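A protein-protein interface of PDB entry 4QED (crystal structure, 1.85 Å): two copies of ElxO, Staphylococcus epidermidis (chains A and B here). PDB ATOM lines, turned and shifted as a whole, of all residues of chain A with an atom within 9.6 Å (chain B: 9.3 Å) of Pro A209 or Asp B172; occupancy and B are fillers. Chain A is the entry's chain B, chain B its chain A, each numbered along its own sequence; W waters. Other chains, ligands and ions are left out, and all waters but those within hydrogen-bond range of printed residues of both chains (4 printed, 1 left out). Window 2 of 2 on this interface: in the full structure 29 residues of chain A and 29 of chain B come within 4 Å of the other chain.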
ATOM      1  N   ILE A 140       3.591  14.909 -12.637  1.00  0.00           N
ATOM      2  CA  ILE A 140       3.315  13.473 -12.432  1.00  0.00           C
ATOM      3  C   ILE A 140       4.612  12.710 -12.134  1.00  0.00           C
ATOM      4  O   ILE A 140       4.603  11.727 -11.384  1.00  0.00           O
ATOM      5  CB  ILE A 140       2.526  12.816 -13.598  1.00  0.00           C
ATOM      6  CG1 ILE A 140       3.230  13.022 -14.954  1.00  0.00           C
ATOM      7  CG2 ILE A 140       1.079  13.317 -13.606  1.00  0.00           C
ATOM      8  CD1 ILE A 140       2.529  12.357 -16.129  1.00  0.00           C
ATOM      9  N   GLY A 183       0.205  16.566 -15.680  1.00  0.00           N
ATOM     10  CA  GLY A 183       0.646  15.587 -16.671  1.00  0.00           C
ATOM     11  C   GLY A 183       1.326  16.346 -17.801  1.00  0.00           C
ATOM     12  O   GLY A 183       1.960  17.386 -17.564  1.00  0.00           O
ATOM     13  N   ILE A 204       1.361  10.928 -27.743  1.00  0.00           N
ATOM     14  CA  ILE A 204       1.738  11.271 -26.367  1.00  0.00           C
ATOM     15  C   ILE A 204       0.561  11.512 -25.418  1.00  0.00           C
ATOM     16  O   ILE A 204       0.713  11.365 -24.205  1.00  0.00           O
ATOM     17  CB  ILE A 204       2.758  12.435 -26.293  1.00  0.00           C
ATOM     18  CG1 ILE A 204       2.541  13.451 -27.419  1.00  0.00           C
ATOM     19  CG2 ILE A 204       4.178  11.893 -26.357  1.00  0.00           C
ATOM     20  CD1 ILE A 204       1.560  14.551 -27.090  1.00  0.00           C
ATOM     21  N   SER A 205      -0.604  11.864 -25.963  1.00  0.00           N
ATOM     22  CA  SER A 205      -1.800  12.081 -25.140  1.00  0.00           C
ATOM     23  C   SER A 205      -2.403  10.770 -24.625  1.00  0.00           C
ATOM     24  O   SER A 205      -3.199  10.775 -23.676  1.00  0.00           O
ATOM     25  CB  SER A 205      -2.853  12.887 -25.899  1.00  0.00           C
ATOM     26  OG  SER A 205      -3.397  12.134 -26.965  1.00  0.00           O
ATOM     27  N   SER A 206      -2.017   9.659 -25.254  1.00  0.00           N
ATOM     28  CA  SER A 206      -2.491   8.326 -24.873  1.00  0.00           C
ATOM     29  C   SER A 206      -1.987   7.858 -23.503  1.00  0.00           C
ATOM     30  O   SER A 206      -2.523   6.902 -22.940  1.00  0.00           O
ATOM     31  CB  SER A 206      -2.123   7.298 -25.951  1.00  0.00           C
ATOM     32  OG  SER A 206      -0.720   7.116 -26.024  1.00  0.00           O
ATOM     33  N   ILE A 207      -0.971   8.526 -22.960  1.00  0.00           N
ATOM     34  CA  ILE A 207      -0.493   8.178 -21.613  1.00  0.00           C
ATOM     35  C   ILE A 207      -1.484   8.587 -20.509  1.00  0.00           C
ATOM     36  O   ILE A 207      -1.493   7.985 -19.433  1.00  0.00           O
ATOM     37  CB  ILE A 207       0.947   8.679 -21.317  1.00  0.00           C
ATOM     38  CG1 ILE A 207       0.980  10.177 -21.016  1.00  0.00           C
ATOM     39  CG2 ILE A 207       1.899   8.323 -22.453  1.00  0.00           C
ATOM     40  CD1 ILE A 207       2.074  10.539 -20.039  1.00  0.00           C
ATOM     41  N   HIS A 208      -2.321   9.589 -20.787  1.00  0.00           N
ATOM     42  CA  HIS A 208      -3.402   9.980 -19.877  1.00  0.00           C
ATOM     43  C   HIS A 208      -4.652   9.148 -20.153  1.00  0.00           C
ATOM     44  O   HIS A 208      -5.057   9.006 -21.314  1.00  0.00           O
ATOM     45  CB  HIS A 208      -3.784  11.457 -20.035  1.00  0.00           C
ATOM     46  CG  HIS A 208      -2.620  12.394 -20.100  1.00  0.00           C
ATOM     47  ND1 HIS A 208      -1.796  12.641 -19.023  1.00  0.00           N
ATOM     48  CD2 HIS A 208      -2.164  13.174 -21.107  1.00  0.00           C
ATOM     49  CE1 HIS A 208      -0.869  13.516 -19.370  1.00  0.00           C
ATOM     50  NE2 HIS A 208      -1.071  13.856 -20.631  1.00  0.00           N
ATOM     51  N   PRO A 209      -5.276   8.602 -19.090  1.00  0.00           N
ATOM     52  CA  PRO A 209      -6.563   7.923 -19.248  1.00  0.00           C
ATOM     53  C   PRO A 209      -7.613   8.763 -19.985  1.00  0.00           C
ATOM     54  O   PRO A 209      -8.421   8.209 -20.724  1.00  0.00           O
ATOM     55  CB  PRO A 209      -6.980   7.650 -17.803  1.00  0.00           C
ATOM     56  CG  PRO A 209      -5.677   7.395 -17.114  1.00  0.00           C
ATOM     57  CD  PRO A 209      -4.656   8.283 -17.790  1.00  0.00           C
ATOM     58  N   MET A 210      -7.594  10.085 -19.813  1.00  0.00           N
ATOM     59  CA  MET A 210      -8.538  10.947 -20.545  1.00  0.00           C
ATOM     60  C   MET A 210      -8.260  11.061 -22.050  1.00  0.00           C
ATOM     61  O   MET A 210      -9.036  11.683 -22.776  1.00  0.00           O
ATOM     62  CB  MET A 210      -8.652  12.332 -19.900  1.00  0.00           C
ATOM     63  CG  MET A 210      -9.399  12.318 -18.574  1.00  0.00           C
ATOM     64  SD  MET A 210      -9.780  13.977 -17.975  1.00  0.00           S
ATOM     65  CE  MET A 210     -11.389  14.243 -18.719  1.00  0.00           C
ATOM     66  N   GLN A 211      -7.160  10.465 -22.507  1.00  0.00           N
ATOM     67  CA  GLN A 211      -6.810  10.420 -23.939  1.00  0.00           C
ATOM     68  C   GLN A 211      -6.786  11.799 -24.618  1.00  0.00           C
ATOM     69  O   GLN A 211      -7.210  11.948 -25.773  1.00  0.00           O
ATOM     70  CB  GLN A 211      -7.743   9.457 -24.696  1.00  0.00           C
ATOM     71  CG  GLN A 211      -7.774   8.043 -24.134  1.00  0.00           C
ATOM     72  CD  GLN A 211      -6.508   7.255 -24.434  1.00  0.00           C
ATOM     73  OE1 GLN A 211      -5.722   6.952 -23.535  1.00  0.00           O
ATOM     74  NE2 GLN A 211      -6.305   6.921 -25.701  1.00  0.00           N
ATOM     75  N   LYS A 212      -6.312  12.802 -23.879  1.00  0.00           N
ATOM     76  CA  LYS A 212      -6.039  14.139 -24.412  1.00  0.00           C
ATOM     77  C   LYS A 212      -4.906  14.771 -23.591  1.00  0.00           C
ATOM     78  O   LYS A 212      -4.540  14.257 -22.529  1.00  0.00           O
ATOM     79  CB  LYS A 212      -7.297  15.013 -24.352  1.00  0.00           C
ATOM     80  CG  LYS A 212      -7.710  15.369 -22.929  1.00  0.00           C
ATOM     81  CD  LYS A 212      -9.111  15.942 -22.852  1.00  0.00           C
ATOM     82  CE  LYS A 212      -9.450  16.270 -21.404  1.00  0.00           C
ATOM     83  NZ  LYS A 212     -10.791  16.891 -21.245  1.00  0.00           N
ATOM     84  N   LEU A 213      -4.357  15.880 -24.076  1.00  0.00           N
ATOM     85  CA  LEU A 213      -3.310  16.584 -23.342  1.00  0.00           C
ATOM     86  C   LEU A 213      -3.926  17.564 -22.366  1.00  0.00           C
ATOM     87  O   LEU A 213      -5.076  17.971 -22.519  1.00  0.00           O
ATOM     88  CB  LEU A 213      -2.373  17.325 -24.299  1.00  0.00           C
ATOM     89  CG  LEU A 213      -1.459  16.482 -25.190  1.00  0.00           C
ATOM     90  CD1 LEU A 213      -0.759  17.391 -26.184  1.00  0.00           C
ATOM     91  CD2 LEU A 213      -0.458  15.703 -24.356  1.00  0.00           C
ATOM     92  N   ILE A 241      -3.154  17.197 -11.903  1.00  0.00           N
ATOM     93  CA  ILE A 241      -3.899  17.780 -13.016  1.00  0.00           C
ATOM     94  C   ILE A 241      -3.370  17.026 -14.231  1.00  0.00           C
ATOM     95  O   ILE A 241      -2.523  17.514 -14.970  1.00  0.00           O
ATOM     96  CB  ILE A 241      -3.701  19.317 -13.097  1.00  0.00           C
ATOM     97  CG1 ILE A 241      -4.043  19.980 -11.743  1.00  0.00           C
ATOM     98  CG2 ILE A 241      -4.575  19.915 -14.200  1.00  0.00           C
ATOM     99  CD1 ILE A 241      -3.781  21.475 -11.683  1.00  0.00           C
ATOM    100  N   ASP A 242      -3.872  15.806 -14.403  1.00  0.00           N
ATOM    101  CA  ASP A 242      -3.152  14.792 -15.170  1.00  0.00           C
ATOM    102  C   ASP A 242      -4.035  13.842 -15.995  1.00  0.00           C
ATOM    103  O   ASP A 242      -3.578  12.769 -16.415  1.00  0.00           O
ATOM    104  CB  ASP A 242      -2.248  13.984 -14.218  1.00  0.00           C
ATOM    105  CG  ASP A 242      -3.028  13.079 -13.258  1.00  0.00           C
ATOM    106  OD1 ASP A 242      -4.271  13.131 -13.226  1.00  0.00           O
ATOM    107  OD2 ASP A 242      -2.376  12.302 -12.521  1.00  0.00           O
ATOM    108  N   GLY A 243      -5.290  14.225 -16.213  1.00  0.00           N
ATOM    109  CA  GLY A 243      -6.235  13.374 -16.963  1.00  0.00           C
ATOM    110  C   GLY A 243      -6.347  11.960 -16.418  1.00  0.00           C
ATOM    111  O   GLY A 243      -6.626  11.013 -17.169  1.00  0.00           O
ATOM    112  N   GLY A 244      -6.108  11.816 -15.115  1.00  0.00           N
ATOM    113  CA  GLY A 244      -6.247  10.526 -14.425  1.00  0.00           C
ATOM    114  C   GLY A 244      -4.982   9.694 -14.341  1.00  0.00           C
ATOM    115  O   GLY A 244      -5.012   8.569 -13.846  1.00  0.00           O
ATOM    116  N   TYR A 245      -3.864  10.239 -14.813  1.00  0.00           N
ATOM    117  CA  TYR A 245      -2.629   9.457 -14.912  1.00  0.00           C
ATOM    118  C   TYR A 245      -2.244   8.755 -13.611  1.00  0.00           C
ATOM    119  O   TYR A 245      -1.980   7.550 -13.615  1.00  0.00           O
ATOM    120  CB  TYR A 245      -1.456  10.306 -15.419  1.00  0.00           C
ATOM    121  CG  TYR A 245      -0.185   9.499 -15.551  1.00  0.00           C
ATOM    122  CD1 TYR A 245       0.145   8.883 -16.757  1.00  0.00           C
ATOM    123  CD2 TYR A 245       0.682   9.334 -14.461  1.00  0.00           C
ATOM    124  CE1 TYR A 245       1.304   8.129 -16.880  1.00  0.00           C
ATOM    125  CE2 TYR A 245       1.840   8.585 -14.575  1.00  0.00           C
ATOM    126  CZ  TYR A 245       2.145   7.986 -15.783  1.00  0.00           C
ATOM    127  OH  TYR A 245       3.294   7.241 -15.899  1.00  0.00           O
ATOM    128  N   LEU A 246      -2.211   9.499 -12.506  1.00  0.00           N
ATOM    129  CA  LEU A 246      -1.718   8.953 -11.239  1.00  0.00           C
ATOM    130  C   LEU A 246      -2.717   8.025 -10.534  1.00  0.00           C
ATOM    131  O   LEU A 246      -2.359   7.363  -9.562  1.00  0.00           O
ATOM    132  CB  LEU A 246      -1.250  10.067 -10.296  1.00  0.00           C
ATOM    133  CG  LEU A 246      -0.009  10.841 -10.770  1.00  0.00           C
ATOM    134  CD1 LEU A 246       0.130  12.155 -10.015  1.00  0.00           C
ATOM    135  CD2 LEU A 246       1.271  10.010 -10.680  1.00  0.00           C
ATOM    136  N   SER A 247      -3.953   7.968 -11.031  1.00  0.00           N
ATOM    137  CA  SER A 247      -4.982   7.103 -10.431  1.00  0.00           C
ATOM    138  C   SER A 247      -4.916   5.659 -10.924  1.00  0.00           C
ATOM    139  O   SER A 247      -5.628   4.783 -10.415  1.00  0.00           O
ATOM    140  CB  SER A 247      -6.370   7.673 -10.677  1.00  0.00           C
ATOM    141  OG  SER A 247      -6.673   7.641 -12.062  1.00  0.00           O
ATOM    142  N   GLN A 248      -4.086   5.418 -11.934  1.00  0.00           N
ATOM    143  CA  GLN A 248      -3.792   4.062 -12.388  1.00  0.00           C
ATOM    144  C   GLN A 248      -2.421   3.654 -11.872  1.00  0.00           C
ATOM    145  O   GLN A 248      -2.138   2.468 -11.738  1.00  0.00           O
ATOM    146  CB  GLN A 248      -3.850   3.942 -13.920  1.00  0.00           C
ATOM    147  CG  GLN A 248      -3.654   5.249 -14.668  1.00  0.00           C
ATOM    148  CD  GLN A 248      -3.149   5.083 -16.091  1.00  0.00           C
ATOM    149  OE1 GLN A 248      -3.701   4.314 -16.880  1.00  0.00           O
ATOM    150  NE2 GLN A 248      -2.104   5.832 -16.434  1.00  0.00           N
ATOM    151  N   GLN B 127     -22.902   8.295 -19.295  1.00  0.00           N
ATOM    152  CA  GLN B 127     -22.330   7.536 -20.428  1.00  0.00           C
ATOM    153  C   GLN B 127     -22.948   7.948 -21.767  1.00  0.00           C
ATOM    154  O   GLN B 127     -22.248   8.132 -22.760  1.00  0.00           O
ATOM    155  CB  GLN B 127     -22.619   6.042 -20.250  1.00  0.00           C
ATOM    156  CG  GLN B 127     -21.471   5.161 -19.794  1.00  0.00           C
ATOM    157  CD  GLN B 127     -21.910   3.719 -19.556  1.00  0.00           C
ATOM    158  OE1 GLN B 127     -23.091   3.382 -19.674  1.00  0.00           O
ATOM    159  NE2 GLN B 127     -20.961   2.861 -19.217  1.00  0.00           N
ATOM    160  N   SER B 130     -21.689  11.437 -22.731  1.00  0.00           N
ATOM    161  CA  SER B 130     -20.239  11.612 -22.621  1.00  0.00           C
ATOM    162  C   SER B 130     -19.837  12.897 -21.886  1.00  0.00           C
ATOM    163  O   SER B 130     -18.947  13.627 -22.331  1.00  0.00           O
ATOM    164  CB  SER B 130     -19.576  11.555 -24.005  1.00  0.00           C
ATOM    165  OG  SER B 130     -19.922  10.355 -24.670  1.00  0.00           O
ATOM    166  N   CYS B 131     -20.500  13.171 -20.767  1.00  0.00           N
ATOM    167  CA  CYS B 131     -20.087  14.257 -19.875  1.00  0.00           C
ATOM    168  C   CYS B 131     -20.755  14.112 -18.522  1.00  0.00           C
ATOM    169  O   CYS B 131     -21.722  13.361 -18.372  1.00  0.00           O
ATOM    170  CB  CYS B 131     -20.383  15.633 -20.479  1.00  0.00           C
ATOM    171  SG  CYS B 131     -22.140  15.990 -20.630  1.00  0.00           S
ATOM    172  N   LYS B 164     -11.324   5.871  -7.875  1.00  0.00           N
ATOM    173  CA  LYS B 164     -10.193   5.689  -8.792  1.00  0.00           C
ATOM    174  C   LYS B 164     -10.517   4.687  -9.899  1.00  0.00           C
ATOM    175  O   LYS B 164     -10.224   4.929 -11.068  1.00  0.00           O
ATOM    176  CB  LYS B 164      -8.938   5.260  -8.031  1.00  0.00           C
ATOM    177  CG  LYS B 164      -8.376   6.314  -7.092  1.00  0.00           C
ATOM    178  CD  LYS B 164      -7.122   5.773  -6.422  1.00  0.00           C
ATOM    179  CE  LYS B 164      -6.304   6.866  -5.759  1.00  0.00           C
ATOM    180  NZ  LYS B 164      -4.967   6.319  -5.379  1.00  0.00           N
ATOM    181  N   GLY B 165     -11.140   3.574  -9.520  1.00  0.00           N
ATOM    182  CA  GLY B 165     -11.584   2.557 -10.466  1.00  0.00           C
ATOM    183  C   GLY B 165     -12.492   3.120 -11.543  1.00  0.00           C
ATOM    184  O   GLY B 165     -12.226   2.933 -12.735  1.00  0.00           O
ATOM    185  N   ALA B 166     -13.560   3.797 -11.124  1.00  0.00           N
ATOM    186  CA  ALA B 166     -14.524   4.399 -12.061  1.00  0.00           C
ATOM    187  C   ALA B 166     -13.892   5.501 -12.905  1.00  0.00           C
ATOM    188  O   ALA B 166     -14.159   5.617 -14.109  1.00  0.00           O
ATOM    189  CB  ALA B 166     -15.742   4.929 -11.312  1.00  0.00           C
ATOM    190  N   ALA B 167     -13.039   6.307 -12.277  1.00  0.00           N
ATOM    191  CA  ALA B 167     -12.348   7.376 -12.991  1.00  0.00           C
ATOM    192  C   ALA B 167     -11.589   6.835 -14.196  1.00  0.00           C
ATOM    193  O   ALA B 167     -11.756   7.337 -15.312  1.00  0.00           O
ATOM    194  CB  ALA B 167     -11.406   8.124 -12.064  1.00  0.00           C
ATOM    195  N   VAL B 168     -10.779   5.804 -13.973  1.00  0.00           N
ATOM    196  CA  VAL B 168      -9.961   5.234 -15.049  1.00  0.00           C
ATOM    197  C   VAL B 168     -10.876   4.591 -16.100  1.00  0.00           C
ATOM    198  O   VAL B 168     -10.607   4.672 -17.304  1.00  0.00           O
ATOM    199  CB  VAL B 168      -8.915   4.217 -14.526  1.00  0.00           C
ATOM    200  CG1 VAL B 168      -8.089   3.659 -15.682  1.00  0.00           C
ATOM    201  CG2 VAL B 168      -7.977   4.870 -13.512  1.00  0.00           C
ATOM    202  N   GLU B 169     -11.962   3.977 -15.638  1.00  0.00           N
ATOM    203  CA  GLU B 169     -12.903   3.308 -16.531  1.00  0.00           C
ATOM    204  C   GLU B 169     -13.694   4.282 -17.421  1.00  0.00           C
ATOM    205  O   GLU B 169     -13.967   3.980 -18.589  1.00  0.00           O
ATOM    206  CB  GLU B 169     -13.846   2.404 -15.729  1.00  0.00           C
ATOM    207  CG  GLU B 169     -14.538   1.340 -16.569  1.00  0.00           C
ATOM    208  CD  GLU B 169     -15.388   0.410 -15.735  1.00  0.00           C
ATOM    209  OE1 GLU B 169     -14.828  -0.487 -15.062  1.00  0.00           O
ATOM    210  OE2 GLU B 169     -16.620   0.585 -15.755  1.00  0.00           O
ATOM    211  N   PHE B 170     -14.046   5.443 -16.876  1.00  0.00           N
ATOM    212  CA  PHE B 170     -14.829   6.438 -17.616  1.00  0.00           C
ATOM    213  C   PHE B 170     -14.037   7.648 -18.126  1.00  0.00           C
ATOM    214  O   PHE B 170     -14.624   8.606 -18.642  1.00  0.00           O
ATOM    215  CB  PHE B 170     -16.036   6.878 -16.773  1.00  0.00           C
ATOM    216  CG  PHE B 170     -17.061   5.793 -16.611  1.00  0.00           C
ATOM    217  CD1 PHE B 170     -18.122   5.686 -17.504  1.00  0.00           C
ATOM    218  CD2 PHE B 170     -16.934   4.840 -15.605  1.00  0.00           C
ATOM    219  CE1 PHE B 170     -19.052   4.665 -17.381  1.00  0.00           C
ATOM    220  CE2 PHE B 170     -17.860   3.816 -15.476  1.00  0.00           C
ATOM    221  CZ  PHE B 170     -18.923   3.728 -16.367  1.00  0.00           C
ATOM    222  N   ALA B 171     -12.713   7.596 -17.994  1.00  0.00           N
ATOM    223  CA  ALA B 171     -11.855   8.730 -18.357  1.00  0.00           C
ATOM    224  C   ALA B 171     -11.957   9.106 -19.832  1.00  0.00           C
ATOM    225  O   ALA B 171     -11.959  10.291 -20.168  1.00  0.00           O
ATOM    226  CB  ALA B 171     -10.406   8.455 -17.971  1.00  0.00           C
ATOM    227  N   ASP B 172     -12.052   8.100 -20.700  1.00  0.00           N
ATOM    228  CA  ASP B 172     -12.161   8.332 -22.141  1.00  0.00           C
ATOM    229  C   ASP B 172     -13.586   8.694 -22.567  1.00  0.00           C
ATOM    230  O   ASP B 172     -13.827   8.975 -23.742  1.00  0.00           O
ATOM    231  CB  ASP B 172     -11.642   7.123 -22.939  1.00  0.00           C
ATOM    232  CG  ASP B 172     -12.601   5.921 -22.913  1.00  0.00           C
ATOM    233  OD1 ASP B 172     -13.499   5.838 -22.041  1.00  0.00           O
ATOM    234  OD2 ASP B 172     -12.440   5.033 -23.776  1.00  0.00           O
ATOM    235  N   LYS B 173     -14.521   8.679 -21.615  1.00  0.00           N
ATOM    236  CA  LYS B 173     -15.908   9.064 -21.884  1.00  0.00           C
ATOM    237  C   LYS B 173     -16.211  10.502 -21.437  1.00  0.00           C
ATOM    238  O   LYS B 173     -17.367  10.922 -21.428  1.00  0.00           O
ATOM    239  CB  LYS B 173     -16.883   8.066 -21.249  1.00  0.00           C
ATOM    240  CG  LYS B 173     -16.748   6.645 -21.786  1.00  0.00           C
ATOM    241  CD  LYS B 173     -17.837   5.731 -21.243  1.00  0.00           C
ATOM    242  CE  LYS B 173     -17.693   4.302 -21.752  1.00  0.00           C
ATOM    243  NZ  LYS B 173     -16.741   3.493 -20.940  1.00  0.00           N
ATOM    244  N   GLY B 174     -15.170  11.243 -21.059  1.00  0.00           N
ATOM    245  CA  GLY B 174     -15.290  12.658 -20.695  1.00  0.00           C
ATOM    246  C   GLY B 174     -15.958  12.943 -19.359  1.00  0.00           C
ATOM    247  O   GLY B 174     -16.414  14.061 -19.108  1.00  0.00           O
ATOM    248  N   ILE B 175     -16.024  11.933 -18.501  1.00  0.00           N
ATOM    249  CA  ILE B 175     -16.646  12.081 -17.195  1.00  0.00           C
ATOM    250  C   ILE B 175     -15.539  12.174 -16.156  1.00  0.00           C
ATOM    251  O   ILE B 175     -14.610  11.375 -16.180  1.00  0.00           O
ATOM    252  CB  ILE B 175     -17.601  10.904 -16.913  1.00  0.00           C
ATOM    253  CG1 ILE B 175     -18.783  10.948 -17.895  1.00  0.00           C
ATOM    254  CG2 ILE B 175     -18.095  10.926 -15.468  1.00  0.00           C
ATOM    255  CD1 ILE B 175     -19.481   9.617 -18.075  1.00  0.00           C
ATOM    256  N   LYS B 176     -15.636  13.163 -15.268  1.00  0.00           N
ATOM    257  CA  LYS B 176     -14.676  13.341 -14.179  1.00  0.00           C
ATOM    258  C   LYS B 176     -15.208  12.722 -12.887  1.00  0.00           C
ATOM    259  O   LYS B 176     -16.351  12.957 -12.489  1.00  0.00           O
ATOM    260  CB  LYS B 176     -14.360  14.825 -13.953  1.00  0.00           C
ATOM    261  CG  LYS B 176     -13.704  15.538 -15.136  1.00  0.00           C
ATOM    262  CD  LYS B 176     -14.744  16.106 -16.090  1.00  0.00           C
ATOM    263  CE  LYS B 176     -14.153  16.270 -17.482  1.00  0.00           C
ATOM    264  NZ  LYS B 176     -15.207  16.376 -18.531  1.00  0.00           N
ATOM    265  N   ILE B 177     -14.378  11.918 -12.235  1.00  0.00           N
ATOM    266  CA  ILE B 177     -14.792  11.263 -11.007  1.00  0.00           C
ATOM    267  C   ILE B 177     -13.692  11.421  -9.965  1.00  0.00           C
ATOM    268  O   ILE B 177     -12.596  10.886 -10.117  1.00  0.00           O
ATOM    269  CB  ILE B 177     -15.117   9.772 -11.240  1.00  0.00           C
ATOM    270  CG1 ILE B 177     -16.222   9.623 -12.307  1.00  0.00           C
ATOM    271  CG2 ILE B 177     -15.519   9.100  -9.936  1.00  0.00           C
ATOM    272  CD1 ILE B 177     -16.464   8.199 -12.752  1.00  0.00           C
ATOM    273  N   ASN B 232     -11.619  20.181 -16.621  1.00  0.00           N
ATOM    274  CA  ASN B 232     -11.492  19.401 -17.844  1.00  0.00           C
ATOM    275  C   ASN B 232     -10.466  18.277 -17.765  1.00  0.00           C
ATOM    276  O   ASN B 232     -10.404  17.439 -18.663  1.00  0.00           O
ATOM    277  CB  ASN B 232     -11.140  20.315 -19.028  1.00  0.00           C
ATOM    278  CG  ASN B 232     -12.239  21.309 -19.347  1.00  0.00           C
ATOM    279  OD1 ASN B 232     -12.004  22.517 -19.373  1.00  0.00           O
ATOM    280  ND2 ASN B 232     -13.445  20.811 -19.578  1.00  0.00           N
ATOM    281  N   PHE B 233      -9.658  18.242 -16.707  1.00  0.00           N
ATOM    282  CA  PHE B 233      -8.487  17.360 -16.721  1.00  0.00           C
ATOM    283  C   PHE B 233      -8.149  16.763 -15.357  1.00  0.00           C
ATOM    284  O   PHE B 233      -7.131  16.094 -15.212  1.00  0.00           O
ATOM    285  CB  PHE B 233      -7.283  18.142 -17.277  1.00  0.00           C
ATOM    286  CG  PHE B 233      -6.214  17.285 -17.907  1.00  0.00           C
ATOM    287  CD1 PHE B 233      -6.513  16.432 -18.971  1.00  0.00           C
ATOM    288  CD2 PHE B 233      -4.889  17.375 -17.474  1.00  0.00           C
ATOM    289  CE1 PHE B 233      -5.515  15.668 -19.566  1.00  0.00           C
ATOM    290  CE2 PHE B 233      -3.888  16.610 -18.063  1.00  0.00           C
ATOM    291  CZ  PHE B 233      -4.204  15.752 -19.113  1.00  0.00           C
ATOM    292  N   THR B 235      -9.190  14.030 -12.734  1.00  0.00           N
ATOM    293  CA  THR B 235     -10.019  12.859 -12.469  1.00  0.00           C
ATOM    294  C   THR B 235      -9.210  11.783 -11.749  1.00  0.00           C
ATOM    295  O   THR B 235      -7.979  11.730 -11.870  1.00  0.00           O
ATOM    296  CB  THR B 235     -10.704  12.328 -13.758  1.00  0.00           C
ATOM    297  OG1 THR B 235     -11.780  11.452 -13.402  1.00  0.00           O
ATOM    298  CG2 THR B 235      -9.720  11.590 -14.665  1.00  0.00           C
ATOM    299  N   GLY B 236      -9.901  10.961 -10.968  1.00  0.00           N
ATOM    300  CA  GLY B 236      -9.252   9.932 -10.167  1.00  0.00           C
ATOM    301  C   GLY B 236      -8.516  10.463  -8.946  1.00  0.00           C
ATOM    302  O   GLY B 236      -7.747   9.736  -8.317  1.00  0.00           O
HETATM  303  O   HOH W   1      -5.252  11.309 -11.133  1.00  0.00           O
HETATM  304  O   HOH W   2     -12.151  12.008 -22.297  1.00  0.00           O
HETATM  305  O   HOH W   3      -6.183  14.571 -11.933  1.00  0.00           O
HETATM  306  O   HOH W   4      -3.406   5.547  -7.691  1.00  0.00           O
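No position is printed for both chains.
The backbone carbonyl oxygen (O) of Gly A244 is in hydrogen-bond range of the side-chain hydroxyl (OG) of Ser A247 (2.6 Å). The side-chain carboxylate (OD2) of Asp A242 sits at hydrogen-bond distance from the backbone NH (N) of Leu A246 (2.8 Å). The backbone carbonyl oxygen of Ile B177 lies within hydrogen-bond range of the backbone NH of Gly B236. The backbone NH (N) of Tyr A245 is in hydrogen-bond range of the side-chain carboxylate (OD1) of Asp A242 (3.3 Å). The backbone carbonyl oxygen of Ile A241 sits at hydrogen-bond distance from the backbone NH of Gly A183 (3.0 Å). The backbone carbonyl oxygen (O) of His A208 sits close to the side-chain amide oxygen (OE1) of Gln A211 (3.1 Å).
Asp B172 touches just one residue of chain A: Pro A209 (3.6 Å). Gly A244 touches one residue of chain B. Of chain A, only Pro A209 and Met A210 come within 4 Å of Ala B171. Printed residues of chain A within 4 Å of Phe B233: His A208 (3.8 Å), Met A210 (3.8 Å), Lys A212 (3.4 Å), Leu A213 (3.7 Å), Ile A241 (3.4 Å), Asp A242 (3.4 Å) and Gly A243 (2.8 Å). Of the printed residues of chain B, Gly A243 touches Phe B233 (2.8 Å) and Thr B235 (3.8 Å). Printed residues of chain A within 4 Å of Val B168: Ser A247 (3.4 Å). Of the printed residues of chain B, Lys A212 touches Asn B232 and Phe B233. Of the printed residues of chain B, Ser A247 touches Val B168 (3.4 Å) and Gly B236 (3.4 Å). Cys B131 touches none of the printed residues of chain A. The nearest residue of chain A that does not touch Asp B172 is Gln A211 (4.2 Å). The nearest printed residue of chain A that does not touch Lys B176 is Lys A212 (5.1 Å).
Of the 20 printed residues of chain A, 10 touch a printed residue of chain B. Among the printed residues, no Asp or Glu carboxylate lies within 4 Å of a Lys or Arg side-chain nitrogen of the other chain.
Water W3 lies within hydrogen-bond range of OD1 of Asp A242 (2.7 Å) and N of Thr B235 (3.2 Å). Water W2 lies within hydrogen-bond range of the backbone carbonyl oxygen of Ala B171, the backbone carbonyl oxygen of Met A210 and the backbone NH of Gly B174. Water W4 bridges the backbone carbonyl oxygen (O) of Leu A246 and the side-chain amino group (NZ) of Lys B164. Water W1 bridges O of Thr B235 (2.9 Å) and OD1 of Asp A242 (2.9 Å).
The backbone carbonyl oxygen (O) of Phe B233 lies within hydrogen-bond range of the backbone NH (N) of Asp A242 (3.4 Å). The side-chain sulfur (SD) of Met A210 lies close to the backbone carbonyl oxygen (O) of Asn B232, 3.6 Å away. The backbone carbonyl oxygen (O) of Asn B232 is in hydrogen-bond range of the side-chain amino group (NZ) of Lys A212. The backbone carbonyl oxygen (O) of Phe B233 lies within hydrogen-bond range of the backbone NH (N) of Gly A243, at 2.8 Å.
His A208 touches Phe B233. O of Pro A209 touches CB of Ala B171, at 3.4 Å. CA of Met A210 touches O of Ala B171 (3.5 Å). Phe B233 touches Met A210. CG2 of Thr B235 touches CG of Met A210, at 3.99 Å. Ile A241 touches Phe B233. CG2 of Thr B235 touches C of Gly A243 (3.8 Å). Gly A244 touches Thr B235 (CA to O, 3.3 Å). Ser A247 touches Val B168 (OG to CG2, 3.4 Å). O of Gly B236 touches CB of Ser A247 (3.4 Å).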
